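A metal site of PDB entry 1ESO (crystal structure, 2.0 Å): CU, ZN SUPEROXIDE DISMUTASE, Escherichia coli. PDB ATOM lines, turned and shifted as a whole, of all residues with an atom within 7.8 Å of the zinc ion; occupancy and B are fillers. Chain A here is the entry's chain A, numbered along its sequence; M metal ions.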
ATOM      1  N   PHE A  47      -9.889  -4.112  -2.766  1.00  0.00           N
ATOM      2  CA  PHE A  47      -9.653  -2.917  -1.945  1.00  0.00           C
ATOM      3  C   PHE A  47      -8.374  -3.148  -1.134  1.00  0.00           C
ATOM      4  O   PHE A  47      -8.356  -3.910  -0.161  1.00  0.00           O
ATOM      5  CB  PHE A  47     -10.866  -2.790  -1.020  1.00  0.00           C
ATOM      6  CG  PHE A  47     -11.067  -1.423  -0.375  1.00  0.00           C
ATOM      7  CD1 PHE A  47     -10.745  -0.243  -1.062  1.00  0.00           C
ATOM      8  CD2 PHE A  47     -11.593  -1.359   0.916  1.00  0.00           C
ATOM      9  CE1 PHE A  47     -10.949   1.001  -0.458  1.00  0.00           C
ATOM     10  CE2 PHE A  47     -11.810  -0.109   1.528  1.00  0.00           C
ATOM     11  CZ  PHE A  47     -11.479   1.067   0.845  1.00  0.00           C
ATOM     12  N   HIS A  48      -7.298  -2.475  -1.533  1.00  0.00           N
ATOM     13  CA  HIS A  48      -5.995  -2.630  -0.855  1.00  0.00           C
ATOM     14  C   HIS A  48      -5.213  -1.325  -0.766  1.00  0.00           C
ATOM     15  O   HIS A  48      -5.442  -0.389  -1.541  1.00  0.00           O
ATOM     16  CB  HIS A  48      -5.080  -3.587  -1.632  1.00  0.00           C
ATOM     17  CG  HIS A  48      -5.804  -4.744  -2.335  1.00  0.00           C
ATOM     18  ND1 HIS A  48      -5.805  -4.883  -3.724  1.00  0.00           N
ATOM     19  CD2 HIS A  48      -6.520  -5.794  -1.854  1.00  0.00           C
ATOM     20  CE1 HIS A  48      -6.493  -5.965  -4.029  1.00  0.00           C
ATOM     21  NE2 HIS A  48      -6.926  -6.519  -2.923  1.00  0.00           N
ATOM     22  N   ILE A  49      -4.312  -1.328   0.195  1.00  0.00           N
ATOM     23  CA  ILE A  49      -3.352  -0.230   0.416  1.00  0.00           C
ATOM     24  C   ILE A  49      -2.065  -0.651  -0.288  1.00  0.00           C
ATOM     25  O   ILE A  49      -1.536  -1.746  -0.055  1.00  0.00           O
ATOM     26  CB  ILE A  49      -3.096  -0.023   1.919  1.00  0.00           C
ATOM     27  CG1 ILE A  49      -4.368   0.296   2.722  1.00  0.00           C
ATOM     28  CG2 ILE A  49      -2.129   1.125   2.202  1.00  0.00           C
ATOM     29  CD1 ILE A  49      -4.072   0.610   4.192  1.00  0.00           C
ATOM     30  N   HIS A  50      -1.564   0.206  -1.153  1.00  0.00           N
ATOM     31  CA  HIS A  50      -0.337  -0.100  -1.921  1.00  0.00           C
ATOM     32  C   HIS A  50       0.869   0.576  -1.227  1.00  0.00           C
ATOM     33  O   HIS A  50       0.705   1.473  -0.383  1.00  0.00           O
ATOM     34  CB  HIS A  50      -0.537   0.290  -3.381  1.00  0.00           C
ATOM     35  CG  HIS A  50      -1.411  -0.742  -4.122  1.00  0.00           C
ATOM     36  ND1 HIS A  50      -0.961  -1.443  -5.243  1.00  0.00           N
ATOM     37  CD2 HIS A  50      -2.681  -1.200  -3.892  1.00  0.00           C
ATOM     38  CE1 HIS A  50      -1.921  -2.258  -5.648  1.00  0.00           C
ATOM     39  NE2 HIS A  50      -2.951  -2.121  -4.855  1.00  0.00           N
ATOM     40  N   GLY A  72       3.308  -2.451  -5.505  1.00  0.00           N
ATOM     41  CA  GLY A  72       2.508  -3.619  -5.067  1.00  0.00           C
ATOM     42  C   GLY A  72       1.760  -3.327  -3.760  1.00  0.00           C
ATOM     43  O   GLY A  72       1.657  -2.168  -3.311  1.00  0.00           O
ATOM     44  N   HIS A  73       1.232  -4.372  -3.164  1.00  0.00           N
ATOM     45  CA  HIS A  73       0.478  -4.272  -1.911  1.00  0.00           C
ATOM     46  C   HIS A  73       1.454  -4.046  -0.746  1.00  0.00           C
ATOM     47  O   HIS A  73       2.506  -4.673  -0.664  1.00  0.00           O
ATOM     48  CB  HIS A  73      -0.304  -5.556  -1.660  1.00  0.00           C
ATOM     49  CG  HIS A  73      -1.480  -5.746  -2.608  1.00  0.00           C
ATOM     50  ND1 HIS A  73      -2.302  -6.870  -2.551  1.00  0.00           N
ATOM     51  CD2 HIS A  73      -1.963  -4.971  -3.618  1.00  0.00           C
ATOM     52  CE1 HIS A  73      -3.227  -6.747  -3.495  1.00  0.00           C
ATOM     53  NE2 HIS A  73      -3.035  -5.617  -4.131  1.00  0.00           N
ATOM     54  N   LEU A  74       1.065  -3.131   0.141  1.00  0.00           N
ATOM     55  CA  LEU A  74       1.844  -2.805   1.345  1.00  0.00           C
ATOM     56  C   LEU A  74       2.156  -4.084   2.109  1.00  0.00           C
ATOM     57  O   LEU A  74       1.268  -4.875   2.444  1.00  0.00           O
ATOM     58  CB  LEU A  74       1.008  -1.894   2.243  1.00  0.00           C
ATOM     59  CG  LEU A  74       1.632  -1.669   3.605  1.00  0.00           C
ATOM     60  CD1 LEU A  74       2.856  -0.747   3.533  1.00  0.00           C
ATOM     61  CD2 LEU A  74       0.671  -1.035   4.601  1.00  0.00           C
ATOM     62  N   ASP A  75       3.419  -4.305   2.408  1.00  0.00           N
ATOM     63  CA  ASP A  75       3.835  -5.560   3.046  1.00  0.00           C
ATOM     64  C   ASP A  75       5.171  -5.365   3.746  1.00  0.00           C
ATOM     65  O   ASP A  75       6.193  -5.945   3.337  1.00  0.00           O
ATOM     66  CB  ASP A  75       3.937  -6.591   1.934  1.00  0.00           C
ATOM     67  CG  ASP A  75       4.319  -7.986   2.368  1.00  0.00           C
ATOM     68  OD1 ASP A  75       4.098  -8.382   3.565  1.00  0.00           O
ATOM     69  OD2 ASP A  75       4.866  -8.771   1.503  1.00  0.00           O
ATOM     70  N   THR A  79       6.008 -10.754   3.562  1.00  0.00           N
ATOM     71  CA  THR A  79       5.396 -12.092   3.617  1.00  0.00           C
ATOM     72  C   THR A  79       5.319 -12.671   2.204  1.00  0.00           C
ATOM     73  O   THR A  79       5.304 -13.894   2.004  1.00  0.00           O
ATOM     74  CB  THR A  79       3.988 -11.989   4.207  1.00  0.00           C
ATOM     75  OG1 THR A  79       3.078 -11.554   3.209  1.00  0.00           O
ATOM     76  CG2 THR A  79       3.886 -11.006   5.373  1.00  0.00           C
ATOM     77  N   GLY A  80       5.253 -11.777   1.237  1.00  0.00           N
ATOM     78  CA  GLY A  80       5.216 -12.133  -0.191  1.00  0.00           C
ATOM     79  C   GLY A  80       3.882 -12.815  -0.581  1.00  0.00           C
ATOM     80  O   GLY A  80       3.692 -13.250  -1.725  1.00  0.00           O
ATOM     81  N   LYS A  81       2.931 -12.925   0.336  1.00  0.00           N
ATOM     82  CA  LYS A  81       1.637 -13.594   0.004  1.00  0.00           C
ATOM     83  C   LYS A  81       0.420 -12.673   0.117  1.00  0.00           C
ATOM     84  O   LYS A  81       0.383 -11.742   0.926  1.00  0.00           O
ATOM     85  CB  LYS A  81       1.293 -14.742   0.960  1.00  0.00           C
ATOM     86  CG  LYS A  81       2.329 -15.861   1.072  1.00  0.00           C
ATOM     87  CD  LYS A  81       2.438 -16.381   2.520  1.00  0.00           C
ATOM     88  CE  LYS A  81       1.952 -17.824   2.716  1.00  0.00           C
ATOM     89  NZ  LYS A  81       1.756 -18.179   4.137  1.00  0.00           N
ATOM     90  N   HIS A  82      -0.569 -12.990  -0.717  1.00  0.00           N
ATOM     91  CA  HIS A  82      -1.850 -12.280  -0.708  1.00  0.00           C
ATOM     92  C   HIS A  82      -2.903 -13.168  -0.051  1.00  0.00           C
ATOM     93  O   HIS A  82      -3.386 -14.141  -0.649  1.00  0.00           O
ATOM     94  CB  HIS A  82      -2.321 -11.960  -2.111  1.00  0.00           C
ATOM     95  CG  HIS A  82      -3.611 -11.152  -2.061  1.00  0.00           C
ATOM     96  ND1 HIS A  82      -3.614  -9.813  -1.673  1.00  0.00           N
ATOM     97  CD2 HIS A  82      -4.903 -11.488  -2.317  1.00  0.00           C
ATOM     98  CE1 HIS A  82      -4.862  -9.383  -1.711  1.00  0.00           C
ATOM     99  NE2 HIS A  82      -5.640 -10.369  -2.089  1.00  0.00           N
ATOM    100  N   GLU A  83      -3.270 -12.803   1.172  1.00  0.00           N
ATOM    101  CA  GLU A  83      -4.190 -13.659   1.934  1.00  0.00           C
ATOM    102  C   GLU A  83      -5.443 -12.974   2.546  1.00  0.00           C
ATOM    103  O   GLU A  83      -6.288 -13.623   3.172  1.00  0.00           O
ATOM    104  CB  GLU A  83      -3.475 -14.309   3.117  1.00  0.00           C
ATOM    105  CG  GLU A  83      -2.203 -15.067   2.707  1.00  0.00           C
ATOM    106  CD  GLU A  83      -1.713 -16.026   3.804  1.00  0.00           C
ATOM    107  OE1 GLU A  83      -2.172 -15.937   5.001  1.00  0.00           O
ATOM    108  OE2 GLU A  83      -0.837 -16.928   3.516  1.00  0.00           O
ATOM    109  N   GLY A  84      -5.610 -11.680   2.376  1.00  0.00           N
ATOM    110  CA  GLY A  84      -6.818 -10.992   2.890  1.00  0.00           C
ATOM    111  C   GLY A  84      -6.594 -10.356   4.272  1.00  0.00           C
ATOM    112  O   GLY A  84      -5.539 -10.536   4.892  1.00  0.00           O
ATOM    113  N   GLY A  89      -0.657 -12.441   5.358  1.00  0.00           N
ATOM    114  CA  GLY A  89       0.062 -11.940   4.168  1.00  0.00           C
ATOM    115  C   GLY A  89       0.221 -10.417   4.226  1.00  0.00           C
ATOM    116  O   GLY A  89       0.413  -9.834   5.308  1.00  0.00           O
ATOM    117  N   HIS A  90       0.128  -9.813   3.046  1.00  0.00           N
ATOM    118  CA  HIS A  90       0.244  -8.354   2.893  1.00  0.00           C
ATOM    119  C   HIS A  90      -0.601  -7.658   3.960  1.00  0.00           C
ATOM    120  O   HIS A  90      -1.790  -7.950   4.131  1.00  0.00           O
ATOM    121  CB  HIS A  90      -0.306  -7.866   1.546  1.00  0.00           C
ATOM    122  CG  HIS A  90       0.239  -8.578   0.310  1.00  0.00           C
ATOM    123  ND1 HIS A  90      -0.605  -8.983  -0.723  1.00  0.00           N
ATOM    124  CD2 HIS A  90       1.491  -8.945  -0.073  1.00  0.00           C
ATOM    125  CE1 HIS A  90       0.125  -9.565  -1.653  1.00  0.00           C
ATOM    126  NE2 HIS A  90       1.385  -9.543  -1.280  1.00  0.00           N
ATOM    127  N   LEU A  91       0.042  -6.744   4.642  1.00  0.00           N
ATOM    128  CA  LEU A  91      -0.601  -5.978   5.704  1.00  0.00           C
ATOM    129  C   LEU A  91      -1.657  -5.033   5.109  1.00  0.00           C
ATOM    130  O   LEU A  91      -2.566  -4.570   5.809  1.00  0.00           O
ATOM    131  CB  LEU A  91       0.436  -5.114   6.412  1.00  0.00           C
ATOM    132  CG  LEU A  91      -0.123  -4.411   7.645  1.00  0.00           C
ATOM    133  CD1 LEU A  91      -0.695  -5.392   8.671  1.00  0.00           C
ATOM    134  CD2 LEU A  91       0.915  -3.571   8.379  1.00  0.00           C
ATOM    135  N   GLY A  92      -1.519  -4.778   3.820  1.00  0.00           N
ATOM    136  CA  GLY A  92      -2.365  -3.821   3.088  1.00  0.00           C
ATOM    137  C   GLY A  92      -3.692  -4.419   2.587  1.00  0.00           C
ATOM    138  O   GLY A  92      -4.560  -3.694   2.060  1.00  0.00           O
ATOM    139  N   ASP A  93      -3.867  -5.710   2.751  1.00  0.00           N
ATOM    140  CA  ASP A  93      -5.096  -6.409   2.296  1.00  0.00           C
ATOM    141  C   ASP A  93      -6.304  -6.018   3.164  1.00  0.00           C
ATOM    142  O   ASP A  93      -6.341  -6.289   4.371  1.00  0.00           O
ATOM    143  CB  ASP A  93      -4.935  -7.933   2.425  1.00  0.00           C
ATOM    144  CG  ASP A  93      -3.799  -8.516   1.570  1.00  0.00           C
ATOM    145  OD1 ASP A  93      -3.114  -7.753   0.782  1.00  0.00           O
ATOM    146  OD2 ASP A  93      -3.524  -9.774   1.644  1.00  0.00           O
ATOM    147  N   LEU A  94      -7.281  -5.398   2.508  1.00  0.00           N
ATOM    148  CA  LEU A  94      -8.543  -4.943   3.139  1.00  0.00           C
ATOM    149  C   LEU A  94      -9.712  -5.825   2.706  1.00  0.00           C
ATOM    150  O   LEU A  94      -9.671  -6.461   1.636  1.00  0.00           O
ATOM    151  CB  LEU A  94      -8.899  -3.528   2.665  1.00  0.00           C
ATOM    152  CG  LEU A  94      -8.309  -2.388   3.489  1.00  0.00           C
ATOM    153  CD1 LEU A  94      -6.953  -2.732   4.119  1.00  0.00           C
ATOM    154  CD2 LEU A  94      -8.060  -1.119   2.661  1.00  0.00           C
ATOM    155  N   ARG A 113      -5.960  -6.050  11.519  1.00  0.00           N
ATOM    156  CA  ARG A 113      -4.493  -6.122  11.679  1.00  0.00           C
ATOM    157  C   ARG A 113      -3.795  -4.754  11.704  1.00  0.00           C
ATOM    158  O   ARG A 113      -2.645  -4.635  12.157  1.00  0.00           O
ATOM    159  CB  ARG A 113      -3.910  -6.969  10.563  1.00  0.00           C
ATOM    160  CG  ARG A 113      -4.212  -8.436  10.801  1.00  0.00           C
ATOM    161  CD  ARG A 113      -3.412  -9.346   9.905  1.00  0.00           C
ATOM    162  NE  ARG A 113      -3.620  -9.047   8.504  1.00  0.00           N
ATOM    163  CZ  ARG A 113      -2.700  -9.186   7.555  1.00  0.00           C
ATOM    164  NH1 ARG A 113      -1.474  -9.623   7.847  1.00  0.00           N
ATOM    165  NH2 ARG A 113      -2.934  -8.907   6.270  1.00  0.00           N
ATOM    166  N   ASP A 132     -11.869  -9.897  -5.153  1.00  0.00           N
ATOM    167  CA  ASP A 132     -10.773 -10.379  -4.300  1.00  0.00           C
ATOM    168  C   ASP A 132     -11.219 -11.627  -3.541  1.00  0.00           C
ATOM    169  O   ASP A 132     -12.077 -11.562  -2.649  1.00  0.00           O
ATOM    170  CB  ASP A 132     -10.352  -9.302  -3.299  1.00  0.00           C
ATOM    171  CG  ASP A 132      -9.002  -9.604  -2.640  1.00  0.00           C
ATOM    172  OD1 ASP A 132      -8.463 -10.764  -2.790  1.00  0.00           O
ATOM    173  OD2 ASP A 132      -8.411  -8.705  -1.936  1.00  0.00           O
ATOM    174  N   MET A 134      -9.120 -13.232  -1.869  1.00  0.00           N
ATOM    175  CA  MET A 134      -8.138 -13.265  -0.773  1.00  0.00           C
ATOM    176  C   MET A 134      -7.080 -14.384  -0.950  1.00  0.00           C
ATOM    177  O   MET A 134      -6.592 -14.975   0.031  1.00  0.00           O
ATOM    178  CB  MET A 134      -8.900 -13.535   0.538  1.00  0.00           C
ATOM    179  CG  MET A 134     -10.106 -12.612   0.708  1.00  0.00           C
ATOM    180  SD  MET A 134      -9.640 -10.895   0.734  1.00  0.00           S
ATOM    181  CE  MET A 134     -11.088  -9.858   0.657  1.00  0.00           C
ATOM    182  N   SER A 135      -6.717 -14.670  -2.188  1.00  0.00           N
ATOM    183  CA  SER A 135      -5.721 -15.721  -2.499  1.00  0.00           C
ATOM    184  C   SER A 135      -4.960 -15.411  -3.794  1.00  0.00           C
ATOM    185  O   SER A 135      -5.388 -14.584  -4.609  1.00  0.00           O
ATOM    186  CB  SER A 135      -6.436 -17.072  -2.678  1.00  0.00           C
ATOM    187  OG  SER A 135      -5.493 -18.091  -2.945  1.00  0.00           O
ATOM    188  N   ASP A 136      -3.826 -16.091  -3.947  1.00  0.00           N
ATOM    189  CA  ASP A 136      -2.994 -15.962  -5.163  1.00  0.00           C
ATOM    190  C   ASP A 136      -3.372 -17.082  -6.148  1.00  0.00           C
ATOM    191  O   ASP A 136      -2.824 -17.189  -7.240  1.00  0.00           O
ATOM    192  CB  ASP A 136      -1.499 -16.032  -4.826  1.00  0.00           C
ATOM    193  CG  ASP A 136      -0.967 -14.692  -4.331  1.00  0.00           C
ATOM    194  OD1 ASP A 136      -1.170 -13.612  -5.013  1.00  0.00           O
ATOM    195  OD2 ASP A 136      -0.337 -14.640  -3.212  1.00  0.00           O
ATOM    196  N   LEU A 141      -2.886 -11.943  -6.622  1.00  0.00           N
ATOM    197  CA  LEU A 141      -3.430 -10.816  -5.858  1.00  0.00           C
ATOM    198  C   LEU A 141      -4.961 -10.847  -5.742  1.00  0.00           C
ATOM    199  O   LEU A 141      -5.604  -9.795  -5.660  1.00  0.00           O
ATOM    200  CB  LEU A 141      -3.079  -9.501  -6.549  1.00  0.00           C
ATOM    201  CG  LEU A 141      -1.612  -9.105  -6.436  1.00  0.00           C
ATOM    202  CD1 LEU A 141      -0.788 -10.100  -5.614  1.00  0.00           C
ATOM    203  CD2 LEU A 141      -0.921  -9.012  -7.798  1.00  0.00           C
ATOM    204  N   GLY A 142      -5.501 -12.055  -5.766  1.00  0.00           N
ATOM    205  CA  GLY A 142      -6.957 -12.301  -5.563  1.00  0.00           C
ATOM    206  C   GLY A 142      -7.832 -12.068  -6.820  1.00  0.00           C
ATOM    207  O   GLY A 142      -9.076 -12.069  -6.732  1.00  0.00           O
HETATM  208 ZN    ZN M   1      -2.406  -8.381  -1.049  1.00  0.00          ZN
HETATM  209 CU    CU M   2      -4.501  -3.531  -4.854  1.00  0.00          CU
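The zinc ion is bound by ND1 of His 90, ND1 of His 82, OD1 of Asp 93 and ND1 of His 73.
N of His 90 sits at hydrogen-bond distance from O of Lys 81 (2.9 Å).
NH2 of Arg 113 is in hydrogen-bond range of O of His 90 (2.6 Å).
The backbone NH (N) of His 90 is in hydrogen-bond range of the side-chain hydroxyl (OG1) of Thr 79, 3.4 Å away.
A ring nitrogen (NE2) of His 82 sits at hydrogen-bond distance from the side-chain carboxylate (OD1) of Asp 132, at 2.9 Å.
OD2 of Asp 136 lies within hydrogen-bond range of N of His 82, at 3.0 Å.
N of Glu 83 lies within hydrogen-bond range of OD2 of Asp 93 (3.1 Å).
OD2 of Asp 93 is in hydrogen-bond range of N of Gly 84, 2.9 Å away.
A ring nitrogen (NE2) of His 73 lies close to a ring nitrogen (ND1) of His 48, 2.9 Å away.
Within 4 Å of the zinc ion: His 73, His 82, His 90 and Asp 93.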
